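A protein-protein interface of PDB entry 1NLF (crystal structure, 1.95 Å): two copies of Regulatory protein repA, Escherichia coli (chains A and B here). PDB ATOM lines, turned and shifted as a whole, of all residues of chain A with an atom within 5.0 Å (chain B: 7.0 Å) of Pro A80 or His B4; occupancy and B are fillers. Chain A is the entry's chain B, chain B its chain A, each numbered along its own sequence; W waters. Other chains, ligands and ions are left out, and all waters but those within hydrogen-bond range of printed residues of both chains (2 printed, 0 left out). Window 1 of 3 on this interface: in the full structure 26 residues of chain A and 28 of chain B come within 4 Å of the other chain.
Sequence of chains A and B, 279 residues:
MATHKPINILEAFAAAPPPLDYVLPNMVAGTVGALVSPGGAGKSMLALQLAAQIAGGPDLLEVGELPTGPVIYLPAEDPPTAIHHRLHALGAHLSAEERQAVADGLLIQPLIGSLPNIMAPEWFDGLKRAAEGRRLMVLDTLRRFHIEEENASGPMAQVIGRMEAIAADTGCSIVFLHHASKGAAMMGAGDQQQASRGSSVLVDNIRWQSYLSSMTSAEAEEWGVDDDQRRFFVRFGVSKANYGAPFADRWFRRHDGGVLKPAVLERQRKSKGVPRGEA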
ATOM      1  N   ASP A  78      24.655   7.885  30.938  1.00  0.00           N
ATOM      2  CA  ASP A  78      24.021   6.692  30.376  1.00  0.00           C
ATOM      3  C   ASP A  78      25.012   5.728  29.724  1.00  0.00           C
ATOM      4  O   ASP A  78      25.893   6.150  28.981  1.00  0.00           O
ATOM      5  CB  ASP A  78      23.003   7.111  29.312  1.00  0.00           C
ATOM      6  CG  ASP A  78      21.576   7.097  29.815  1.00  0.00           C
ATOM      7  OD1 ASP A  78      20.731   7.752  29.171  1.00  0.00           O
ATOM      8  OD2 ASP A  78      21.290   6.426  30.831  1.00  0.00           O
ATOM      9  N   PRO A  79      24.887   4.417  29.998  1.00  0.00           N
ATOM     10  CA  PRO A  79      25.820   3.483  29.361  1.00  0.00           C
ATOM     11  C   PRO A  79      25.478   3.488  27.867  1.00  0.00           C
ATOM     12  O   PRO A  79      24.313   3.639  27.504  1.00  0.00           O
ATOM     13  CB  PRO A  79      25.495   2.153  30.045  1.00  0.00           C
ATOM     14  CG  PRO A  79      24.051   2.291  30.381  1.00  0.00           C
ATOM     15  CD  PRO A  79      23.964   3.708  30.898  1.00  0.00           C
ATOM     16  N   PRO A  80      26.483   3.338  26.987  1.00  0.00           N
ATOM     17  CA  PRO A  80      26.254   3.340  25.535  1.00  0.00           C
ATOM     18  C   PRO A  80      25.096   2.474  25.028  1.00  0.00           C
ATOM     19  O   PRO A  80      24.340   2.891  24.148  1.00  0.00           O
ATOM     20  CB  PRO A  80      27.600   2.890  24.978  1.00  0.00           C
ATOM     21  CG  PRO A  80      28.566   3.489  25.963  1.00  0.00           C
ATOM     22  CD  PRO A  80      27.914   3.149  27.286  1.00  0.00           C
ATOM     23  N   THR A  81      24.952   1.272  25.578  1.00  0.00           N
ATOM     24  CA  THR A  81      23.882   0.378  25.135  1.00  0.00           C
ATOM     25  C   THR A  81      22.479   0.940  25.383  1.00  0.00           C
ATOM     26  O   THR A  81      21.553   0.665  24.621  1.00  0.00           O
ATOM     27  CB  THR A  81      24.011  -1.012  25.797  1.00  0.00           C
ATOM     28  OG1 THR A  81      24.029  -0.877  27.223  1.00  0.00           O
ATOM     29  CG2 THR A  81      25.291  -1.685  25.339  1.00  0.00           C
ATOM     30  N   ALA A  82      22.316   1.724  26.444  1.00  0.00           N
ATOM     31  CA  ALA A  82      21.013   2.318  26.734  1.00  0.00           C
ATOM     32  C   ALA A  82      20.703   3.387  25.687  1.00  0.00           C
ATOM     33  O   ALA A  82      19.541   3.609  25.334  1.00  0.00           O
ATOM     34  CB  ALA A  82      21.008   2.930  28.130  1.00  0.00           C
ATOM     35  N   ILE A  83      21.748   4.042  25.193  1.00  0.00           N
ATOM     36  CA  ILE A  83      21.591   5.079  24.174  1.00  0.00           C
ATOM     37  C   ILE A  83      21.203   4.429  22.845  1.00  0.00           C
ATOM     38  O   ILE A  83      20.407   4.976  22.083  1.00  0.00           O
ATOM     39  CB  ILE A  83      22.898   5.879  23.967  1.00  0.00           C
ATOM     40  CG1 ILE A  83      23.366   6.484  25.296  1.00  0.00           C
ATOM     41  CG2 ILE A  83      22.670   6.986  22.945  1.00  0.00           C
ATOM     42  CD1 ILE A  83      22.350   7.401  25.945  1.00  0.00           C
ATOM     43  N   HIS A  84      21.768   3.258  22.568  1.00  0.00           N
ATOM     44  CA  HIS A  84      21.448   2.546  21.333  1.00  0.00           C
ATOM     45  C   HIS A  84      19.956   2.251  21.312  1.00  0.00           C
ATOM     46  O   HIS A  84      19.284   2.449  20.297  1.00  0.00           O
ATOM     47  CB  HIS A  84      22.218   1.223  21.260  1.00  0.00           C
ATOM     48  CG  HIS A  84      23.705   1.383  21.235  1.00  0.00           C
ATOM     49  ND1 HIS A  84      24.563   0.416  21.713  1.00  0.00           N
ATOM     50  CD2 HIS A  84      24.489   2.381  20.761  1.00  0.00           C
ATOM     51  CE1 HIS A  84      25.812   0.810  21.534  1.00  0.00           C
ATOM     52  NE2 HIS A  84      25.795   1.999  20.959  1.00  0.00           N
ATOM     53  N   GLN A 109      28.592  11.496  21.405  1.00  0.00           N
ATOM     54  CA  GLN A 109      29.835  10.970  21.963  1.00  0.00           C
ATOM     55  C   GLN A 109      29.644  10.611  23.434  1.00  0.00           C
ATOM     56  O   GLN A 109      29.548  11.488  24.294  1.00  0.00           O
ATOM     57  CB  GLN A 109      30.949  12.015  21.814  1.00  0.00           C
ATOM     58  CG  GLN A 109      32.264  11.666  22.503  1.00  0.00           C
ATOM     59  CD  GLN A 109      33.056  10.596  21.779  1.00  0.00           C
ATOM     60  OE1 GLN A 109      34.101  10.158  22.256  1.00  0.00           O
ATOM     61  NE2 GLN A 109      32.567  10.175  20.620  1.00  0.00           N
ATOM     62  N   PRO A 110      29.563   9.308  23.740  1.00  0.00           N
ATOM     63  CA  PRO A 110      29.383   8.874  25.130  1.00  0.00           C
ATOM     64  C   PRO A 110      30.584   9.304  25.978  1.00  0.00           C
ATOM     65  O   PRO A 110      31.722   9.236  25.512  1.00  0.00           O
ATOM     66  CB  PRO A 110      29.283   7.353  25.003  1.00  0.00           C
ATOM     67  CG  PRO A 110      28.695   7.170  23.627  1.00  0.00           C
ATOM     68  CD  PRO A 110      29.466   8.163  22.815  1.00  0.00           C
ATOM     69  N   LEU A 111      30.329   9.747  27.207  1.00  0.00           N
ATOM     70  CA  LEU A 111      31.394  10.181  28.111  1.00  0.00           C
ATOM     71  C   LEU A 111      31.301   9.537  29.492  1.00  0.00           C
ATOM     72  O   LEU A 111      31.932   9.989  30.450  1.00  0.00           O
ATOM     73  CB  LEU A 111      31.377  11.709  28.266  1.00  0.00           C
ATOM     74  CG  LEU A 111      31.827  12.542  27.057  1.00  0.00           C
ATOM     75  CD1 LEU A 111      31.810  14.036  27.432  1.00  0.00           C
ATOM     76  CD2 LEU A 111      33.233  12.129  26.640  1.00  0.00           C
ATOM     77  N   ILE A 112      30.518   8.475  29.612  1.00  0.00           N
ATOM     78  CA  ILE A 112      30.404   7.835  30.911  1.00  0.00           C
ATOM     79  C   ILE A 112      31.777   7.318  31.336  1.00  0.00           C
ATOM     80  O   ILE A 112      32.453   6.618  30.583  1.00  0.00           O
ATOM     81  CB  ILE A 112      29.365   6.687  30.877  1.00  0.00           C
ATOM     82  CG1 ILE A 112      29.240   6.062  32.269  1.00  0.00           C
ATOM     83  CG2 ILE A 112      29.739   5.678  29.796  1.00  0.00           C
ATOM     84  CD1 ILE A 112      28.019   5.159  32.427  1.00  0.00           C
ATOM     85  N   SER A 114      34.436   8.995  31.589  1.00  0.00           N
ATOM     86  CA  SER A 114      35.514   9.795  31.000  1.00  0.00           C
ATOM     87  C   SER A 114      35.975  10.926  31.917  1.00  0.00           C
ATOM     88  O   SER A 114      37.045  11.498  31.716  1.00  0.00           O
ATOM     89  CB  SER A 114      35.069  10.372  29.654  1.00  0.00           C
ATOM     90  OG  SER A 114      34.779   9.330  28.735  1.00  0.00           O
ATOM     91  N   ALA B   2      37.976   6.360  30.943  1.00  0.00           N
ATOM     92  CA  ALA B   2      37.357   5.604  29.820  1.00  0.00           C
ATOM     93  C   ALA B   2      37.076   6.494  28.610  1.00  0.00           C
ATOM     94  O   ALA B   2      36.718   7.664  28.756  1.00  0.00           O
ATOM     95  CB  ALA B   2      36.064   4.948  30.289  1.00  0.00           C
ATOM     96  N   THR B   3      37.249   5.932  27.420  1.00  0.00           N
ATOM     97  CA  THR B   3      37.003   6.653  26.176  1.00  0.00           C
ATOM     98  C   THR B   3      36.035   5.831  25.332  1.00  0.00           C
ATOM     99  O   THR B   3      36.087   4.600  25.338  1.00  0.00           O
ATOM    100  CB  THR B   3      38.301   6.869  25.376  1.00  0.00           C
ATOM    101  OG1 THR B   3      38.906   5.598  25.098  1.00  0.00           O
ATOM    102  CG2 THR B   3      39.275   7.734  26.165  1.00  0.00           C
ATOM    103  N   HIS B   4      35.160   6.516  24.604  1.00  0.00           N
ATOM    104  CA  HIS B   4      34.166   5.846  23.774  1.00  0.00           C
ATOM    105  C   HIS B   4      34.160   6.376  22.348  1.00  0.00           C
ATOM    106  O   HIS B   4      34.413   7.557  22.113  1.00  0.00           O
ATOM    107  CB  HIS B   4      32.770   6.060  24.361  1.00  0.00           C
ATOM    108  CG  HIS B   4      32.640   5.647  25.793  1.00  0.00           C
ATOM    109  ND1 HIS B   4      32.298   4.367  26.174  1.00  0.00           N
ATOM    110  CD2 HIS B   4      32.789   6.354  26.937  1.00  0.00           C
ATOM    111  CE1 HIS B   4      32.237   4.305  27.493  1.00  0.00           C
ATOM    112  NE2 HIS B   4      32.531   5.497  27.980  1.00  0.00           N
ATOM    113  N   LYS B   5      33.858   5.502  21.396  1.00  0.00           N
ATOM    114  CA  LYS B   5      33.779   5.932  20.012  1.00  0.00           C
ATOM    115  C   LYS B   5      32.378   6.506  19.816  1.00  0.00           C
ATOM    116  O   LYS B   5      31.442   6.133  20.528  1.00  0.00           O
ATOM    117  CB  LYS B   5      34.023   4.756  19.061  1.00  0.00           C
ATOM    118  CG  LYS B   5      33.136   3.548  19.293  1.00  0.00           C
ATOM    119  CD  LYS B   5      33.570   2.385  18.413  1.00  0.00           C
ATOM    120  CE  LYS B   5      32.771   1.126  18.712  1.00  0.00           C
ATOM    121  NZ  LYS B   5      33.234  -0.031  17.895  1.00  0.00           N
ATOM    122  N   PRO B   6      32.219   7.445  18.871  1.00  0.00           N
ATOM    123  CA  PRO B   6      30.901   8.039  18.628  1.00  0.00           C
ATOM    124  C   PRO B   6      29.882   6.948  18.289  1.00  0.00           C
ATOM    125  O   PRO B   6      30.243   5.910  17.732  1.00  0.00           O
ATOM    126  CB  PRO B   6      31.158   8.971  17.444  1.00  0.00           C
ATOM    127  CG  PRO B   6      32.599   9.356  17.625  1.00  0.00           C
ATOM    128  CD  PRO B   6      33.237   8.043  17.991  1.00  0.00           C
ATOM    129  N   ILE B   7      28.618   7.187  18.619  1.00  0.00           N
ATOM    130  CA  ILE B   7      27.558   6.217  18.336  1.00  0.00           C
ATOM    131  C   ILE B   7      27.252   6.182  16.843  1.00  0.00           C
ATOM    132  O   ILE B   7      27.202   7.226  16.195  1.00  0.00           O
ATOM    133  CB  ILE B   7      26.232   6.583  19.058  1.00  0.00           C
ATOM    134  CG1 ILE B   7      26.408   6.521  20.582  1.00  0.00           C
ATOM    135  CG2 ILE B   7      25.111   5.653  18.590  1.00  0.00           C
ATOM    136  CD1 ILE B   7      26.620   5.137  21.142  1.00  0.00           C
ATOM    137  N   LEU B  20      19.686  -5.280  26.689  1.00  0.00           N
ATOM    138  CA  LEU B  20      20.583  -4.768  27.720  1.00  0.00           C
ATOM    139  C   LEU B  20      21.079  -5.924  28.589  1.00  0.00           C
ATOM    140  O   LEU B  20      20.358  -6.896  28.820  1.00  0.00           O
ATOM    141  CB  LEU B  20      19.867  -3.734  28.600  1.00  0.00           C
ATOM    142  CG  LEU B  20      19.465  -2.407  27.945  1.00  0.00           C
ATOM    143  CD1 LEU B  20      18.746  -1.537  28.961  1.00  0.00           C
ATOM    144  CD2 LEU B  20      20.705  -1.688  27.419  1.00  0.00           C
ATOM    145  N   GLY B  30      28.574  -2.746  33.603  1.00  0.00           N
ATOM    146  CA  GLY B  30      29.504  -1.702  33.206  1.00  0.00           C
ATOM    147  C   GLY B  30      29.236  -0.370  33.890  1.00  0.00           C
ATOM    148  O   GLY B  30      29.791   0.658  33.501  1.00  0.00           O
ATOM    149  N   ALA B 168      33.448   1.513  33.331  1.00  0.00           N
ATOM    150  CA  ALA B 168      33.276   1.772  31.905  1.00  0.00           C
ATOM    151  C   ALA B 168      34.445   1.274  31.053  1.00  0.00           C
ATOM    152  O   ALA B 168      34.253   0.768  29.945  1.00  0.00           O
ATOM    153  CB  ALA B 168      33.074   3.271  31.677  1.00  0.00           C
ATOM    154  N   ASP B 169      35.658   1.415  31.569  1.00  0.00           N
ATOM    155  CA  ASP B 169      36.836   1.002  30.824  1.00  0.00           C
ATOM    156  C   ASP B 169      37.091  -0.503  30.848  1.00  0.00           C
ATOM    157  O   ASP B 169      37.595  -1.058  29.873  1.00  0.00           O
ATOM    158  CB  ASP B 169      38.066   1.738  31.352  1.00  0.00           C
ATOM    159  CG  ASP B 169      39.295   1.505  30.494  1.00  0.00           C
ATOM    160  OD1 ASP B 169      39.254   1.845  29.292  1.00  0.00           O
ATOM    161  OD2 ASP B 169      40.301   0.984  31.019  1.00  0.00           O
HETATM  162  O   HOH W   1      35.881   9.248  20.044  1.00  0.00           O
HETATM  163  O   HOH W   2      34.888   9.028  25.887  1.00  0.00           O
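The side-chain hydroxyl of Ser A114 is in hydrogen-bond range of the backbone carbonyl oxygen of Ala B2 (2.6 Å). OE1 of Gln A109 sits close to O of His B4 (2.6 Å). O of Ile A112 is in hydrogen-bond range of NE2 of His B4. The side-chain amide nitrogen of Gln A109 lies close to the backbone nitrogen of Pro B6, 3.3 Å away.
The backbone carbonyl oxygen of Pro A80 sits close to a ring nitrogen (ND1) of His A84 (3.5 Å). The backbone carbonyl oxygen (O) of Leu A111 sits close to the side-chain hydroxyl (OG) of Ser A114, at 3.4 Å.
Pro A80 touches His B4. Thr A81 touches Leu B20 (OG1 to CD2, 3.4 Å). Leu B20 touches Ala A82. NE2 of His A84 touches CD1 of Ile B7, at 3.2 Å. C of Lys B5 touches NE2 of Gln A109 (3.8 Å). Pro A110 touches His B4. Pro A110 touches Lys B5 (CD to O, 3.6 Å). Ile B7 touches Pro A110. Ala B2 touches Ile A112. O of Ile A112 touches CB of Ala B168 (3.6 Å).
Pro A80 touches one residue of chain B. Of the printed residues of chain B, Gln A109 touches His B4 (2.6 Å), Lys B5 (3.8 Å) and Pro B6 (3.1 Å). Leu A111 touches none of the printed residues of chain B. Of the printed residues of chain B, Ser A114 touches Ala B2 (2.6 Å). Of the printed residues of chain A, His B4 touches Pro A80, Gln A109, Pro A110 and Ile A112. Of the printed residues of chain A, Lys B5 touches Gln A109 (3.8 Å) and Pro A110 (3.6 Å). Printed residues of chain A within 4 Å of Ala B168: Ile A112. Asp B169 touches none of the printed residues of chain A. The nearest residue of chain B that does not touch Pro A80 is Ile B7 (4.4 Å).
Of the 12 printed residues of chain A, 8 touch a printed residue of chain B. Of the 10 printed residues of chain B, 7 touch a printed residue of chain A. Hydrophobic or aromatic side chains of chain B within 4 Å of the printed part of chain A: Ala B2, His B4, Pro B6, Ile B7, Leu B20 and Ala B168.
No position is printed for both chains. Of the 14 pairs that touch across the chains among the printed residues, none has its exchanged pair printed and touching as well.
Water W2 lies within hydrogen-bond range of N of His B4, OG of Ser A114 and O of Pro A110. Water W1 bridges the side-chain amide oxygen of Gln A109 (3.0 Å) and the backbone carbonyl oxygen of His B4 (3.0 Å).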
